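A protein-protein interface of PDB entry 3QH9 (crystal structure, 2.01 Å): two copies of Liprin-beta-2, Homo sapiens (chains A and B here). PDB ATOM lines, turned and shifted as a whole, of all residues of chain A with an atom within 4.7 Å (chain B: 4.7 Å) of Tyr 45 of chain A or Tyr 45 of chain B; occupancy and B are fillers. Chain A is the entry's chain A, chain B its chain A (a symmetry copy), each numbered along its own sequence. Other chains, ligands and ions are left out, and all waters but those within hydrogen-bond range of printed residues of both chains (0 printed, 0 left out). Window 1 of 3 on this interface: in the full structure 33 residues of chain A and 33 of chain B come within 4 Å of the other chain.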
ATOM      1  N   GLU A  41      -5.148 -23.590  15.777  1.00  0.00           N
ATOM      2  CA  GLU A  41      -3.962 -22.796  16.027  1.00  0.00           C
ATOM      3  C   GLU A  41      -3.739 -21.605  14.999  1.00  0.00           C
ATOM      4  O   GLU A  41      -3.398 -20.480  15.405  1.00  0.00           O
ATOM      5  CB  GLU A  41      -2.754 -23.718  16.133  1.00  0.00           C
ATOM      6  CG  GLU A  41      -1.468 -22.967  16.358  1.00  0.00           C
ATOM      7  CD  GLU A  41      -0.441 -23.773  17.105  1.00  0.00           C
ATOM      8  OE1 GLU A  41      -0.653 -25.010  17.239  1.00  0.00           O
ATOM      9  OE2 GLU A  41       0.574 -23.156  17.542  1.00  0.00           O
ATOM     10  N   ARG A  42      -3.945 -21.840  13.701  1.00  0.00           N
ATOM     11  CA  ARG A  42      -3.886 -20.755  12.707  1.00  0.00           C
ATOM     12  C   ARG A  42      -4.892 -19.608  13.016  1.00  0.00           C
ATOM     13  O   ARG A  42      -4.522 -18.436  12.974  1.00  0.00           O
ATOM     14  CB  ARG A  42      -4.074 -21.297  11.281  1.00  0.00           C
ATOM     15  CG  ARG A  42      -4.184 -20.229  10.213  1.00  0.00           C
ATOM     16  CD  ARG A  42      -4.202 -20.824   8.829  1.00  0.00           C
ATOM     17  NE  ARG A  42      -5.439 -21.551   8.493  1.00  0.00           N
ATOM     18  CZ  ARG A  42      -5.602 -22.248   7.371  1.00  0.00           C
ATOM     19  NH1 ARG A  42      -4.620 -22.322   6.496  1.00  0.00           N
ATOM     20  NH2 ARG A  42      -6.734 -22.874   7.122  1.00  0.00           N
ATOM     21  N   ASN A  43      -6.141 -19.937  13.332  1.00  0.00           N
ATOM     22  CA  ASN A  43      -7.137 -18.911  13.595  1.00  0.00           C
ATOM     23  C   ASN A  43      -6.745 -18.010  14.779  1.00  0.00           C
ATOM     24  O   ASN A  43      -6.997 -16.797  14.779  1.00  0.00           O
ATOM     25  CB  ASN A  43      -8.520 -19.522  13.856  1.00  0.00           C
ATOM     26  CG  ASN A  43      -9.648 -18.463  13.863  1.00  0.00           C
ATOM     27  OD1 ASN A  43     -10.581 -18.527  14.682  1.00  0.00           O
ATOM     28  ND2 ASN A  43      -9.559 -17.487  12.947  1.00  0.00           N
ATOM     29  N   GLN A  44      -6.096 -18.595  15.772  1.00  0.00           N
ATOM     30  CA  GLN A  44      -5.761 -17.834  16.950  1.00  0.00           C
ATOM     31  C   GLN A  44      -4.425 -17.122  16.833  1.00  0.00           C
ATOM     32  O   GLN A  44      -4.187 -16.157  17.542  1.00  0.00           O
ATOM     33  CB  GLN A  44      -5.780 -18.724  18.185  1.00  0.00           C
ATOM     34  CG  GLN A  44      -4.531 -19.585  18.439  1.00  0.00           C
ATOM     35  CD  GLN A  44      -4.658 -20.370  19.756  1.00  0.00           C
ATOM     36  OE1 GLN A  44      -4.467 -21.595  19.790  1.00  0.00           O
ATOM     37  NE2 GLN A  44      -5.012 -19.666  20.837  1.00  0.00           N
ATOM     38  N   TYR A  45      -3.527 -17.641  16.017  1.00  0.00           N
ATOM     39  CA  TYR A  45      -2.355 -16.886  15.610  1.00  0.00           C
ATOM     40  C   TYR A  45      -2.799 -15.610  14.810  1.00  0.00           C
ATOM     41  O   TYR A  45      -2.285 -14.525  15.031  1.00  0.00           O
ATOM     42  CB  TYR A  45      -1.383 -17.771  14.798  1.00  0.00           C
ATOM     43  CG  TYR A  45      -0.126 -18.295  15.565  1.00  0.00           C
ATOM     44  CD1 TYR A  45       0.666 -17.453  16.370  1.00  0.00           C
ATOM     45  CD2 TYR A  45       0.303 -19.632  15.419  1.00  0.00           C
ATOM     46  CE1 TYR A  45       1.830 -17.951  17.051  1.00  0.00           C
ATOM     47  CE2 TYR A  45       1.464 -20.126  16.096  1.00  0.00           C
ATOM     48  CZ  TYR A  45       2.224 -19.278  16.909  1.00  0.00           C
ATOM     49  OH  TYR A  45       3.360 -19.773  17.547  1.00  0.00           O
ATOM     50  N   GLU A  46      -3.789 -15.735  13.925  1.00  0.00           N
ATOM     51  CA  GLU A  46      -4.278 -14.581  13.157  1.00  0.00           C
ATOM     52  C   GLU A  46      -4.874 -13.478  14.064  1.00  0.00           C
ATOM     53  O   GLU A  46      -4.682 -12.273  13.830  1.00  0.00           O
ATOM     54  CB  GLU A  46      -5.207 -15.061  12.049  1.00  0.00           C
ATOM     55  CG  GLU A  46      -6.529 -14.438  12.019  1.00  0.00           C
ATOM     56  CD  GLU A  46      -7.558 -15.182  11.150  1.00  0.00           C
ATOM     57  OE1 GLU A  46      -8.663 -14.582  11.059  1.00  0.00           O
ATOM     58  OE2 GLU A  46      -7.281 -16.321  10.603  1.00  0.00           O
ATOM     59  N   TRP A  47      -5.541 -13.872  15.139  1.00  0.00           N
ATOM     60  CA  TRP A  47      -6.086 -12.891  16.067  1.00  0.00           C
ATOM     61  C   TRP A  47      -5.013 -12.306  17.042  1.00  0.00           C
ATOM     62  O   TRP A  47      -5.045 -11.095  17.319  1.00  0.00           O
ATOM     63  CB  TRP A  47      -7.252 -13.501  16.837  1.00  0.00           C
ATOM     64  CG  TRP A  47      -8.514 -13.553  16.033  1.00  0.00           C
ATOM     65  CD1 TRP A  47      -9.074 -14.642  15.472  1.00  0.00           C
ATOM     66  CD2 TRP A  47      -9.357 -12.445  15.689  1.00  0.00           C
ATOM     67  NE1 TRP A  47     -10.219 -14.296  14.792  1.00  0.00           N
ATOM     68  CE2 TRP A  47     -10.404 -12.950  14.890  1.00  0.00           C
ATOM     69  CE3 TRP A  47      -9.305 -11.078  15.945  1.00  0.00           C
ATOM     70  CZ2 TRP A  47     -11.422 -12.142  14.381  1.00  0.00           C
ATOM     71  CZ3 TRP A  47     -10.307 -10.267  15.430  1.00  0.00           C
ATOM     72  CH2 TRP A  47     -11.359 -10.809  14.664  1.00  0.00           C
ATOM     73  N   LYS A  48      -4.072 -13.120  17.547  1.00  0.00           N
ATOM     74  CA  LYS A  48      -2.903 -12.583  18.305  1.00  0.00           C
ATOM     75  C   LYS A  48      -2.012 -11.669  17.461  1.00  0.00           C
ATOM     76  O   LYS A  48      -1.467 -10.678  17.928  1.00  0.00           O
ATOM     77  CB  LYS A  48      -2.062 -13.743  18.880  1.00  0.00           C
ATOM     78  CG  LYS A  48      -0.882 -13.376  19.850  1.00  0.00           C
ATOM     79  CD  LYS A  48      -1.195 -12.306  20.942  1.00  0.00           C
ATOM     80  CE  LYS A  48       0.087 -11.564  21.513  1.00  0.00           C
ATOM     81  NZ  LYS A  48      -0.088 -10.051  21.779  1.00  0.00           N
ATOM     82  N   LEU A  49      -1.878 -11.967  16.196  1.00  0.00           N
ATOM     83  CA  LEU A  49      -1.106 -11.061  15.364  1.00  0.00           C
ATOM     84  C   LEU A  49      -1.867  -9.742  15.292  1.00  0.00           C
ATOM     85  O   LEU A  49      -1.320  -8.654  15.425  1.00  0.00           O
ATOM     86  CB  LEU A  49      -0.930 -11.666  13.971  1.00  0.00           C
ATOM     87  CG  LEU A  49      -0.175 -10.792  13.007  1.00  0.00           C
ATOM     88  CD1 LEU A  49       1.300 -10.670  13.473  1.00  0.00           C
ATOM     89  CD2 LEU A  49      -0.335 -11.481  11.690  1.00  0.00           C
ATOM     90  N   GLU B  41       2.388 -22.796   7.413  1.00  0.00           N
ATOM     91  CA  GLU B  41       1.747 -21.571   7.845  1.00  0.00           C
ATOM     92  C   GLU B  41       1.936 -21.239   9.389  1.00  0.00           C
ATOM     93  O   GLU B  41       2.210 -20.082   9.754  1.00  0.00           O
ATOM     94  CB  GLU B  41       0.285 -21.593   7.421  1.00  0.00           C
ATOM     95  CG  GLU B  41      -0.468 -20.367   7.865  1.00  0.00           C
ATOM     96  CD  GLU B  41      -1.620 -20.026   6.960  1.00  0.00           C
ATOM     97  OE1 GLU B  41      -1.975 -20.894   6.115  1.00  0.00           O
ATOM     98  OE2 GLU B  41      -2.164 -18.893   7.114  1.00  0.00           O
ATOM     99  N   ARG B  42       1.809 -22.233  10.272  1.00  0.00           N
ATOM    100  CA  ARG B  42       2.099 -22.028  11.701  1.00  0.00           C
ATOM    101  C   ARG B  42       3.550 -21.525  11.950  1.00  0.00           C
ATOM    102  O   ARG B  42       3.751 -20.577  12.709  1.00  0.00           O
ATOM    103  CB  ARG B  42       1.797 -23.297  12.514  1.00  0.00           C
ATOM    104  CG  ARG B  42       2.215 -23.224  13.968  1.00  0.00           C
ATOM    105  CD  ARG B  42       1.749 -24.428  14.745  1.00  0.00           C
ATOM    106  NE  ARG B  42       2.453 -25.680  14.412  1.00  0.00           N
ATOM    107  CZ  ARG B  42       2.106 -26.870  14.897  1.00  0.00           C
ATOM    108  NH1 ARG B  42       1.077 -26.973  15.712  1.00  0.00           N
ATOM    109  NH2 ARG B  42       2.777 -27.955  14.567  1.00  0.00           N
ATOM    110  N   ASN B  43       4.545 -22.138  11.316  1.00  0.00           N
ATOM    111  CA  ASN B  43       5.925 -21.737  11.535  1.00  0.00           C
ATOM    112  C   ASN B  43       6.173 -20.268  11.152  1.00  0.00           C
ATOM    113  O   ASN B  43       6.944 -19.552  11.804  1.00  0.00           O
ATOM    114  CB  ASN B  43       6.902 -22.636  10.764  1.00  0.00           C
ATOM    115  CG  ASN B  43       8.374 -22.419  11.188  1.00  0.00           C
ATOM    116  OD1 ASN B  43       9.288 -22.420  10.347  1.00  0.00           O
ATOM    117  ND2 ASN B  43       8.597 -22.232  12.497  1.00  0.00           N
ATOM    118  N   GLN B  44       5.490 -19.808  10.117  1.00  0.00           N
ATOM    119  CA  GLN B  44       5.723 -18.464   9.651  1.00  0.00           C
ATOM    120  C   GLN B  44       4.856 -17.435  10.355  1.00  0.00           C
ATOM    121  O   GLN B  44       5.194 -16.263  10.369  1.00  0.00           O
ATOM    122  CB  GLN B  44       5.524 -18.379   8.142  1.00  0.00           C
ATOM    123  CG  GLN B  44       4.076 -18.257   7.640  1.00  0.00           C
ATOM    124  CD  GLN B  44       4.033 -18.102   6.109  1.00  0.00           C
ATOM    125  OE1 GLN B  44       3.314 -18.835   5.414  1.00  0.00           O
ATOM    126  NE2 GLN B  44       4.830 -17.166   5.583  1.00  0.00           N
ATOM    127  N   TYR B  45       3.706 -17.848  10.856  1.00  0.00           N
ATOM    128  CA  TYR B  45       2.959 -17.030  11.795  1.00  0.00           C
ATOM    129  C   TYR B  45       3.805 -16.812  13.100  1.00  0.00           C
ATOM    130  O   TYR B  45       3.881 -15.711  13.618  1.00  0.00           O
ATOM    131  CB  TYR B  45       1.579 -17.657  12.096  1.00  0.00           C
ATOM    132  CG  TYR B  45       0.357 -17.008  11.372  1.00  0.00           C
ATOM    133  CD1 TYR B  45       0.168 -15.613  11.322  1.00  0.00           C
ATOM    134  CD2 TYR B  45      -0.651 -17.811  10.794  1.00  0.00           C
ATOM    135  CE1 TYR B  45      -0.976 -15.037  10.668  1.00  0.00           C
ATOM    136  CE2 TYR B  45      -1.789 -17.238  10.144  1.00  0.00           C
ATOM    137  CZ  TYR B  45      -1.946 -15.848  10.087  1.00  0.00           C
ATOM    138  OH  TYR B  45      -3.070 -15.307   9.465  1.00  0.00           O
ATOM    139  N   GLU B  46       4.481 -17.853  13.591  1.00  0.00           N
ATOM    140  CA  GLU B  46       5.317 -17.722  14.793  1.00  0.00           C
ATOM    141  C   GLU B  46       6.480 -16.720  14.597  1.00  0.00           C
ATOM    142  O   GLU B  46       6.824 -15.941  15.502  1.00  0.00           O
ATOM    143  CB  GLU B  46       5.744 -19.104  15.273  1.00  0.00           C
ATOM    144  CG  GLU B  46       7.182 -19.294  15.447  1.00  0.00           C
ATOM    145  CD  GLU B  46       7.614 -20.766  15.568  1.00  0.00           C
ATOM    146  OE1 GLU B  46       8.842 -20.910  15.814  1.00  0.00           O
ATOM    147  OE2 GLU B  46       6.769 -21.733  15.403  1.00  0.00           O
ATOM    148  N   TRP B  47       7.052 -16.681  13.403  1.00  0.00           N
ATOM    149  CA  TRP B  47       8.118 -15.729  13.128  1.00  0.00           C
ATOM    150  C   TRP B  47       7.592 -14.285  12.838  1.00  0.00           C
ATOM    151  O   TRP B  47       8.213 -13.312  13.299  1.00  0.00           O
ATOM    152  CB  TRP B  47       8.983 -16.237  11.979  1.00  0.00           C
ATOM    153  CG  TRP B  47       9.943 -17.305  12.406  1.00  0.00           C
ATOM    154  CD1 TRP B  47       9.853 -18.625  12.152  1.00  0.00           C
ATOM    155  CD2 TRP B  47      11.133 -17.124  13.185  1.00  0.00           C
ATOM    156  NE1 TRP B  47      10.910 -19.295  12.722  1.00  0.00           N
ATOM    157  CE2 TRP B  47      11.699 -18.402  13.382  1.00  0.00           C
ATOM    158  CE3 TRP B  47      11.748 -16.019  13.765  1.00  0.00           C
ATOM    159  CZ2 TRP B  47      12.882 -18.601  14.097  1.00  0.00           C
ATOM    160  CZ3 TRP B  47      12.916 -16.212  14.488  1.00  0.00           C
ATOM    161  CH2 TRP B  47      13.476 -17.498  14.637  1.00  0.00           C
ATOM    162  N   LYS B  48       6.475 -14.127  12.112  1.00  0.00           N
ATOM    163  CA  LYS B  48       5.809 -12.797  11.985  1.00  0.00           C
ATOM    164  C   LYS B  48       5.313 -12.247  13.324  1.00  0.00           C
ATOM    165  O   LYS B  48       5.357 -11.053  13.595  1.00  0.00           O
ATOM    166  CB  LYS B  48       4.633 -12.882  10.990  1.00  0.00           C
ATOM    167  CG  LYS B  48       3.913 -11.542  10.596  1.00  0.00           C
ATOM    168  CD  LYS B  48       4.841 -10.330  10.276  1.00  0.00           C
ATOM    169  CE  LYS B  48       4.142  -8.913  10.434  1.00  0.00           C
ATOM    170  NZ  LYS B  48       5.024  -7.805  11.054  1.00  0.00           N
ATOM    171  N   LEU B  49       4.866 -13.110  14.196  1.00  0.00           N
ATOM    172  CA  LEU B  49       4.473 -12.612  15.503  1.00  0.00           C
ATOM    173  C   LEU B  49       5.728 -12.095  16.195  1.00  0.00           C
ATOM    174  O   LEU B  49       5.763 -11.026  16.791  1.00  0.00           O
ATOM    175  CB  LEU B  49       3.829 -13.740  16.311  1.00  0.00           C
ATOM    176  CG  LEU B  49       3.415 -13.347  17.702  1.00  0.00           C
ATOM    177  CD1 LEU B  49       2.249 -12.328  17.622  1.00  0.00           C
ATOM    178  CD2 LEU B  49       3.041 -14.641  18.349  1.00  0.00           C
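The side-chain carboxylate (OE1) of Glu 41 of chain A lies within salt-bridge range of the guanidinium group (NH1) of Arg 42 of chain B (3.0 Å).
The guanidinium group (NH1) of Arg 42 of chain A lies within salt-bridge range of the side-chain carboxylate (OE1) of Glu 41 of chain B, at 3.0 Å.
The side-chain amide nitrogen of Asn 43 of chain A lies within hydrogen-bond range of the side-chain carboxylate of Glu 46 of chain A.
The side-chain amide nitrogen (ND2) of Asn 43 of chain B lies within hydrogen-bond range of the side-chain carboxylate (OE2) of Glu 46 of chain B, at 3.5 Å.
Among the printed residues, pairs that only touch across the chains: Tyr 45 of chain A with Glu 46 of chain B, Glu 46 of chain A with Tyr 45 of chain B, Leu 49 of chain A with Tyr 45 of chain B, Tyr 45 of chain A with Leu 49 of chain B, Arg 42 of chain A with Tyr 45 of chain B, Tyr 45 of chain A with Arg 42 of chain B, Tyr 45 of chain A with Tyr 45 of chain B, Leu 49 of chain A with Lys 48 of chain B and Lys 48 of chain A with Leu 49 of chain B.
Of the printed residues of chain B, Tyr 45 of chain A touches Arg 42 (3.8 Å), Tyr 45 (3.9 Å), Glu 46 (3.4 Å) and Leu 49 (3.8 Å).
Of the printed residues of chain A, Tyr 45 of chain B touches Arg 42 (3.8 Å), Tyr 45 (3.9 Å), Glu 46 (3.4 Å) and Leu 49 (3.8 Å).
Of the printed residues of chain A, Lys 48 of chain B touches Leu 49.
Printed residues of chain A within 4 Å of Arg 42 of chain B: Glu 41 and Tyr 45.
Of the printed residues of chain B, Glu 46 of chain A touches Tyr 45.
Of the printed residues of chain B, Arg 42 of chain A touches Glu 41 and Tyr 45.
Printed residues of chain A within 4 Å of Glu 46 of chain B: Tyr 45.
Trp 47 of chain A touches none of the printed residues of chain B.
Asn 43 of chain B touches none of the printed residues of chain A.
The nearest printed residue of chain B that does not touch Tyr 45 of chain A is Glu 41 of chain B (6.0 Å).
The nearest printed residue of chain B that does not touch Leu 49 of chain A is Leu 49 of chain B (4.2 Å).
Printed residues of chain A that touch a printed residue of chain B: Glu 41, Arg 42, Tyr 45, Glu 46, Lys 48 and Leu 49.
Arg 42 of chain A touches Tyr 45 of chain B, and with the chains exchanged Tyr 45 of chain A touches Arg 42 of chain B.
Tyr 45 of chain B touches its own counterpart, Tyr 45 of chain A.
Tyr 45 of chain A touches Glu 46 of chain B, and with the chains exchanged Glu 46 of chain A touches Tyr 45 of chain B.
Tyr 45 of chain A touches Leu 49 of chain B, and with the chains exchanged Leu 49 of chain A touches Tyr 45 of chain B.
9 positions are printed for both chains.
Of the 11 pairs that touch across the chains among the printed residues, 11 have their exchanged pair printed and touching as well.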
